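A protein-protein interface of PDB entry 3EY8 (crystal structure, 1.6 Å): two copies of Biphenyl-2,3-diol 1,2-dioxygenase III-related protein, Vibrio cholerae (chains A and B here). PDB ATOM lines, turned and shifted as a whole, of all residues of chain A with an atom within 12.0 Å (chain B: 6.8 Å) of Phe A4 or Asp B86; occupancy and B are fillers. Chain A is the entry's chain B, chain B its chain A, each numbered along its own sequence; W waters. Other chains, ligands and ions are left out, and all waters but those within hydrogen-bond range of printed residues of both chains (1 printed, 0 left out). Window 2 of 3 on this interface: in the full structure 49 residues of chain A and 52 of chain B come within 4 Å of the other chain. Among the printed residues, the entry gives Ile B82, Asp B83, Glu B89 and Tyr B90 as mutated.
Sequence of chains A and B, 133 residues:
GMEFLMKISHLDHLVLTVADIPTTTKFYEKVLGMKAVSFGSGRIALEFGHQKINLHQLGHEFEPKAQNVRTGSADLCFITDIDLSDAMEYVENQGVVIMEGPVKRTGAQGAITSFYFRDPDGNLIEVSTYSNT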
ATOM      1  N   MET A   2      -5.218 -15.811 -19.326  1.00  0.00           N
ATOM      2  CA  MET A   2      -5.970 -15.394 -18.149  1.00  0.00           C
ATOM      3  C   MET A   2      -6.652 -14.050 -18.366  1.00  0.00           C
ATOM      4  O   MET A   2      -6.174 -13.008 -17.913  1.00  0.00           O
ATOM      5  CB  MET A   2      -5.070 -15.343 -16.913  1.00  0.00           C
ATOM      6  CG  MET A   2      -5.027 -16.634 -16.111  1.00  0.00           C
ATOM      7  SD  MET A   2      -6.139 -16.599 -14.505  1.00  0.00           S
ATOM      8  CE  MET A   2      -7.734 -17.436 -15.138  1.00  0.00           C
ATOM      9  N   GLU A   3      -7.767 -14.087 -19.081  1.00  0.00           N
ATOM     10  CA  GLU A   3      -8.646 -12.939 -19.188  1.00  0.00           C
ATOM     11  C   GLU A   3      -9.136 -12.603 -17.781  1.00  0.00           C
ATOM     12  O   GLU A   3      -9.195 -13.480 -16.919  1.00  0.00           O
ATOM     13  CB  GLU A   3      -9.812 -13.290 -20.114  1.00  0.00           C
ATOM     14  CG  GLU A   3     -11.036 -12.404 -20.001  1.00  0.00           C
ATOM     15  CD  GLU A   3     -12.146 -12.850 -20.937  1.00  0.00           C
ATOM     16  OE1 GLU A   3     -11.855 -13.097 -22.128  1.00  0.00           O
ATOM     17  OE2 GLU A   3     -13.307 -12.955 -20.481  1.00  0.00           O
ATOM     18  N   PHE A   4      -9.457 -11.340 -17.528  1.00  0.00           N
ATOM     19  CA  PHE A   4     -10.003 -10.968 -16.227  1.00  0.00           C
ATOM     20  C   PHE A   4     -10.984  -9.809 -16.329  1.00  0.00           C
ATOM     21  O   PHE A   4     -10.986  -9.066 -17.314  1.00  0.00           O
ATOM     22  CB  PHE A   4      -8.890 -10.646 -15.217  1.00  0.00           C
ATOM     23  CG  PHE A   4      -8.226  -9.312 -15.438  1.00  0.00           C
ATOM     24  CD1 PHE A   4      -8.697  -8.173 -14.806  1.00  0.00           C
ATOM     25  CD2 PHE A   4      -7.121  -9.203 -16.265  1.00  0.00           C
ATOM     26  CE1 PHE A   4      -8.085  -6.949 -15.003  1.00  0.00           C
ATOM     27  CE2 PHE A   4      -6.507  -7.983 -16.466  1.00  0.00           C
ATOM     28  CZ  PHE A   4      -6.992  -6.854 -15.834  1.00  0.00           C
ATOM     29  N   LEU A   5     -11.825  -9.675 -15.309  1.00  0.00           N
ATOM     30  CA  LEU A   5     -12.747  -8.548 -15.212  1.00  0.00           C
ATOM     31  C   LEU A   5     -12.255  -7.592 -14.140  1.00  0.00           C
ATOM     32  O   LEU A   5     -11.861  -8.013 -13.058  1.00  0.00           O
ATOM     33  CB  LEU A   5     -14.154  -9.031 -14.849  1.00  0.00           C
ATOM     34  CG  LEU A   5     -14.840  -9.945 -15.869  1.00  0.00           C
ATOM     35  CD1 LEU A   5     -16.180 -10.458 -15.335  1.00  0.00           C
ATOM     36  CD2 LEU A   5     -15.027  -9.225 -17.192  1.00  0.00           C
ATOM     37  N   MET A   6     -12.280  -6.297 -14.435  1.00  0.00           N
ATOM     38  CA  MET A   6     -11.951  -5.308 -13.417  1.00  0.00           C
ATOM     39  C   MET A   6     -13.018  -5.293 -12.322  1.00  0.00           C
ATOM     40  O   MET A   6     -14.217  -5.300 -12.612  1.00  0.00           O
ATOM     41  CB  MET A   6     -11.815  -3.921 -14.047  1.00  0.00           C
ATOM     42  CG  MET A   6     -11.406  -2.856 -13.058  1.00  0.00           C
ATOM     43  SD  MET A   6      -9.689  -3.220 -12.233  1.00  0.00           S
ATOM     44  CE  MET A   6      -9.777  -1.842 -10.851  1.00  0.00           C
ATOM     45  N   LYS A   7     -12.576  -5.267 -11.066  1.00  0.00           N
ATOM     46  CA  LYS A   7     -13.480  -5.282  -9.916  1.00  0.00           C
ATOM     47  C   LYS A   7     -12.922  -4.476  -8.762  1.00  0.00           C
ATOM     48  O   LYS A   7     -11.710  -4.442  -8.535  1.00  0.00           O
ATOM     49  CB  LYS A   7     -13.734  -6.714  -9.442  1.00  0.00           C
ATOM     50  CG  LYS A   7     -14.564  -7.551 -10.407  1.00  0.00           C
ATOM     51  CD  LYS A   7     -16.022  -7.129 -10.362  1.00  0.00           C
ATOM     52  CE  LYS A   7     -16.837  -7.870 -11.402  1.00  0.00           C
ATOM     53  NZ  LYS A   7     -18.288  -7.631 -11.203  1.00  0.00           N
ATOM     54  N   ILE A   8     -13.820  -3.827  -8.034  1.00  0.00           N
ATOM     55  CA  ILE A   8     -13.466  -3.122  -6.813  1.00  0.00           C
ATOM     56  C   ILE A   8     -14.083  -3.878  -5.638  1.00  0.00           C
ATOM     57  O   ILE A   8     -15.242  -4.296  -5.693  1.00  0.00           O
ATOM     58  CB  ILE A   8     -13.989  -1.661  -6.839  1.00  0.00           C
ATOM     59  CG1 ILE A   8     -13.231  -0.844  -7.889  1.00  0.00           C
ATOM     60  CG2 ILE A   8     -13.892  -1.028  -5.445  1.00  0.00           C
ATOM     61  CD1 ILE A   8     -11.715  -0.737  -7.650  1.00  0.00           C
ATOM     62  N   SER A   9     -13.305  -4.057  -4.577  1.00  0.00           N
ATOM     63  CA  SER A   9     -13.747  -4.796  -3.409  1.00  0.00           C
ATOM     64  C   SER A   9     -14.532  -3.923  -2.433  1.00  0.00           C
ATOM     65  O   SER A   9     -15.612  -4.300  -1.976  1.00  0.00           O
ATOM     66  CB  SER A   9     -12.538  -5.412  -2.697  1.00  0.00           C
ATOM     67  OG  SER A   9     -12.889  -5.877  -1.406  1.00  0.00           O
ATOM     68  N   ILE B  82      -7.633  -7.339  -7.454  1.00  0.00           N
ATOM     69  CA  ILE B  82      -6.905  -7.605  -8.696  1.00  0.00           C
ATOM     70  C   ILE B  82      -5.478  -7.071  -8.574  1.00  0.00           C
ATOM     71  O   ILE B  82      -5.256  -6.034  -7.957  1.00  0.00           O
ATOM     72  CB  ILE B  82      -7.612  -6.957  -9.889  1.00  0.00           C
ATOM     73  CG1 ILE B  82      -8.939  -7.676 -10.165  1.00  0.00           C
ATOM     74  CG2 ILE B  82      -6.733  -6.992 -11.125  1.00  0.00           C
ATOM     75  CD1 ILE B  82      -9.850  -6.924 -11.079  1.00  0.00           C
ATOM     76  N   ASP B  83      -4.509  -7.790  -9.136  1.00  0.00           N
ATOM     77  CA  ASP B  83      -3.125  -7.325  -9.118  1.00  0.00           C
ATOM     78  C   ASP B  83      -3.074  -5.865  -9.575  1.00  0.00           C
ATOM     79  O   ASP B  83      -3.624  -5.522 -10.619  1.00  0.00           O
ATOM     80  CB  ASP B  83      -2.252  -8.185 -10.035  1.00  0.00           C
ATOM     81  CG  ASP B  83      -0.856  -7.620 -10.196  1.00  0.00           C
ATOM     82  OD1 ASP B  83      -0.003  -7.866  -9.318  1.00  0.00           O
ATOM     83  OD2 ASP B  83      -0.609  -6.920 -11.197  1.00  0.00           O
ATOM     84  N   LEU B  84      -2.412  -5.005  -8.806  1.00  0.00           N
ATOM     85  CA  LEU B  84      -2.487  -3.576  -9.087  1.00  0.00           C
ATOM     86  C   LEU B  84      -1.941  -3.217 -10.470  1.00  0.00           C
ATOM     87  O   LEU B  84      -2.478  -2.336 -11.140  1.00  0.00           O
ATOM     88  CB  LEU B  84      -1.787  -2.751  -8.005  1.00  0.00           C
ATOM     89  CG  LEU B  84      -2.204  -1.276  -8.010  1.00  0.00           C
ATOM     90  CD1 LEU B  84      -3.650  -1.133  -7.505  1.00  0.00           C
ATOM     91  CD2 LEU B  84      -1.248  -0.453  -7.178  1.00  0.00           C
ATOM     92  N   SER B  85      -0.871  -3.883 -10.898  1.00  0.00           N
ATOM     93  CA  SER B  85      -0.289  -3.568 -12.200  1.00  0.00           C
ATOM     94  C   SER B  85      -1.265  -3.933 -13.321  1.00  0.00           C
ATOM     95  O   SER B  85      -1.384  -3.220 -14.318  1.00  0.00           O
ATOM     96  CB  SER B  85       1.065  -4.263 -12.383  1.00  0.00           C
ATOM     97  OG  SER B  85       0.902  -5.651 -12.585  1.00  0.00           O
ATOM     98  N   ASP B  86      -1.977  -5.040 -13.146  1.00  0.00           N
ATOM     99  CA  ASP B  86      -3.003  -5.435 -14.100  1.00  0.00           C
ATOM    100  C   ASP B  86      -4.164  -4.441 -14.094  1.00  0.00           C
ATOM    101  O   ASP B  86      -4.671  -4.061 -15.152  1.00  0.00           O
ATOM    102  CB  ASP B  86      -3.514  -6.842 -13.796  1.00  0.00           C
ATOM    103  CG  ASP B  86      -2.495  -7.927 -14.132  1.00  0.00           C
ATOM    104  OD1 ASP B  86      -1.460  -7.632 -14.776  1.00  0.00           O
ATOM    105  OD2 ASP B  86      -2.738  -9.085 -13.743  1.00  0.00           O
ATOM    106  N   ALA B  87      -4.586  -4.020 -12.907  1.00  0.00           N
ATOM    107  CA  ALA B  87      -5.633  -3.010 -12.805  1.00  0.00           C
ATOM    108  C   ALA B  87      -5.247  -1.707 -13.502  1.00  0.00           C
ATOM    109  O   ALA B  87      -6.056  -1.108 -14.200  1.00  0.00           O
ATOM    110  CB  ALA B  87      -5.985  -2.745 -11.349  1.00  0.00           C
ATOM    111  N   MET B  88      -4.008  -1.276 -13.305  1.00  0.00           N
ATOM    112  CA  MET B  88      -3.559  -0.015 -13.880  1.00  0.00           C
ATOM    113  C   MET B  88      -3.515  -0.110 -15.397  1.00  0.00           C
ATOM    114  O   MET B  88      -3.940   0.807 -16.096  1.00  0.00           O
ATOM    115  CB  MET B  88      -2.185   0.348 -13.323  1.00  0.00           C
ATOM    116  CG  MET B  88      -1.952   1.835 -13.218  1.00  0.00           C
ATOM    117  SD  MET B  88      -0.240   2.219 -12.375  1.00  0.00           S
ATOM    118  CE  MET B  88       0.888   1.951 -13.951  1.00  0.00           C
ATOM    119  N   GLU B  89      -3.019  -1.231 -15.910  1.00  0.00           N
ATOM    120  CA  GLU B  89      -2.972  -1.440 -17.350  1.00  0.00           C
ATOM    121  C   GLU B  89      -4.378  -1.408 -17.938  1.00  0.00           C
ATOM    122  O   GLU B  89      -4.606  -0.794 -18.983  1.00  0.00           O
ATOM    123  CB  GLU B  89      -2.290  -2.760 -17.695  1.00  0.00           C
ATOM    124  CG  GLU B  89      -2.176  -2.989 -19.190  1.00  0.00           C
ATOM    125  CD  GLU B  89      -1.441  -4.265 -19.530  1.00  0.00           C
ATOM    126  OE1 GLU B  89      -1.504  -5.219 -18.727  1.00  0.00           O
ATOM    127  OE2 GLU B  89      -0.806  -4.314 -20.605  1.00  0.00           O
ATOM    128  N   TYR B  90      -5.318  -2.062 -17.260  1.00  0.00           N
ATOM    129  CA  TYR B  90      -6.712  -2.064 -17.682  1.00  0.00           C
ATOM    130  C   TYR B  90      -7.288  -0.655 -17.750  1.00  0.00           C
ATOM    131  O   TYR B  90      -7.923  -0.287 -18.735  1.00  0.00           O
ATOM    132  CB  TYR B  90      -7.573  -2.918 -16.740  1.00  0.00           C
ATOM    133  CG  TYR B  90      -9.049  -2.876 -17.088  1.00  0.00           C
ATOM    134  CD1 TYR B  90      -9.576  -3.719 -18.058  1.00  0.00           C
ATOM    135  CD2 TYR B  90      -9.910  -1.975 -16.462  1.00  0.00           C
ATOM    136  CE1 TYR B  90     -10.922  -3.679 -18.391  1.00  0.00           C
ATOM    137  CE2 TYR B  90     -11.257  -1.926 -16.786  1.00  0.00           C
ATOM    138  CZ  TYR B  90     -11.755  -2.789 -17.753  1.00  0.00           C
ATOM    139  OH  TYR B  90     -13.085  -2.755 -18.087  1.00  0.00           O
ATOM    140  N   VAL B  91      -7.093   0.119 -16.686  1.00  0.00           N
ATOM    141  CA  VAL B  91      -7.613   1.481 -16.638  1.00  0.00           C
ATOM    142  C   VAL B  91      -7.005   2.308 -17.764  1.00  0.00           C
ATOM    143  O   VAL B  91      -7.708   3.053 -18.446  1.00  0.00           O
ATOM    144  CB  VAL B  91      -7.362   2.135 -15.252  1.00  0.00           C
ATOM    145  CG1 VAL B  91      -7.637   3.628 -15.303  1.00  0.00           C
ATOM    146  CG2 VAL B  91      -8.231   1.455 -14.185  1.00  0.00           C
ATOM    147  N   PHE B 115      -2.630   3.793  -7.380  1.00  0.00           N
ATOM    148  CA  PHE B 115      -2.519   4.693  -8.519  1.00  0.00           C
ATOM    149  C   PHE B 115      -3.737   5.611  -8.530  1.00  0.00           C
ATOM    150  O   PHE B 115      -4.748   5.305  -7.889  1.00  0.00           O
ATOM    151  CB  PHE B 115      -2.306   3.961  -9.861  1.00  0.00           C
ATOM    152  CG  PHE B 115      -3.466   3.111 -10.314  1.00  0.00           C
ATOM    153  CD1 PHE B 115      -4.436   3.628 -11.173  1.00  0.00           C
ATOM    154  CD2 PHE B 115      -3.561   1.777  -9.931  1.00  0.00           C
ATOM    155  CE1 PHE B 115      -5.487   2.832 -11.616  1.00  0.00           C
ATOM    156  CE2 PHE B 115      -4.612   0.984 -10.378  1.00  0.00           C
ATOM    157  CZ  PHE B 115      -5.572   1.511 -11.219  1.00  0.00           C
HETATM  158  O   HOH W   1     -13.684  -5.551 -16.996  1.00  0.00           O
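The side-chain carboxylate (OD2) of Asp B83 lies within hydrogen-bond range of the backbone NH (N) of Asp B86, 3.0 Å away.
Among the printed residues, merely in contact across the chains: Phe A4 with Asp B86, Leu A5 with Ile B82, Met A6 with Ile B82, Met A6 with Ala B87, Met A6 with Tyr B90 and Lys A7 with Ile B82.
Met A2 touches none of the printed residues of chain B. Phe A4 touches just one residue of chain B: Asp B86. Of the printed residues of chain B, Leu A5 touches Ile B82. Of the printed residues of chain B, Met A6 touches Ile B82 (3.5 Å), Ala B87 (3.8 Å) and Tyr B90 (3.4 Å). Printed residues of chain B within 4 Å of Lys A7: Ile B82 (3.2 Å). Ser A9 touches none of the printed residues of chain B. Of chain A, only Leu A5 (3.0 Å), Met A6 (3.5 Å) and Lys A7 (3.2 Å) come within 4 Å of Ile B82. No residue of chain A comes within 4 Å of Asp B83. No residue of chain A comes within 4 Å of Leu B84. Asp B86 touches one residue of chain A. Of chain A, only Met A6 comes within 4 Å of Ala B87. Tyr B90 touches one residue of chain A. The nearest residue of chain A that does not touch Asp B86 is Met A6 (5.9 Å).
Of the 11 printed residues of chain B, 4 touch a printed residue of chain A. Printed residues of chain B that touch a printed residue of chain A: Ile B82, Asp B86, Ala B87 and Tyr B90. Among the printed residues, 6 pairs touch across the chains. Among the printed residues, no Asp or Glu carboxylate lies within 4 Å of a Lys or Arg side-chain nitrogen of the other chain.
No position is printed for both chains. Of the 6 pairs that touch across the chains among the printed residues, none has its exchanged pair printed and touching as well.
Water W1 bridges N of Met A6 (3.0 Å) and OH of Tyr B90 (3.1 Å).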
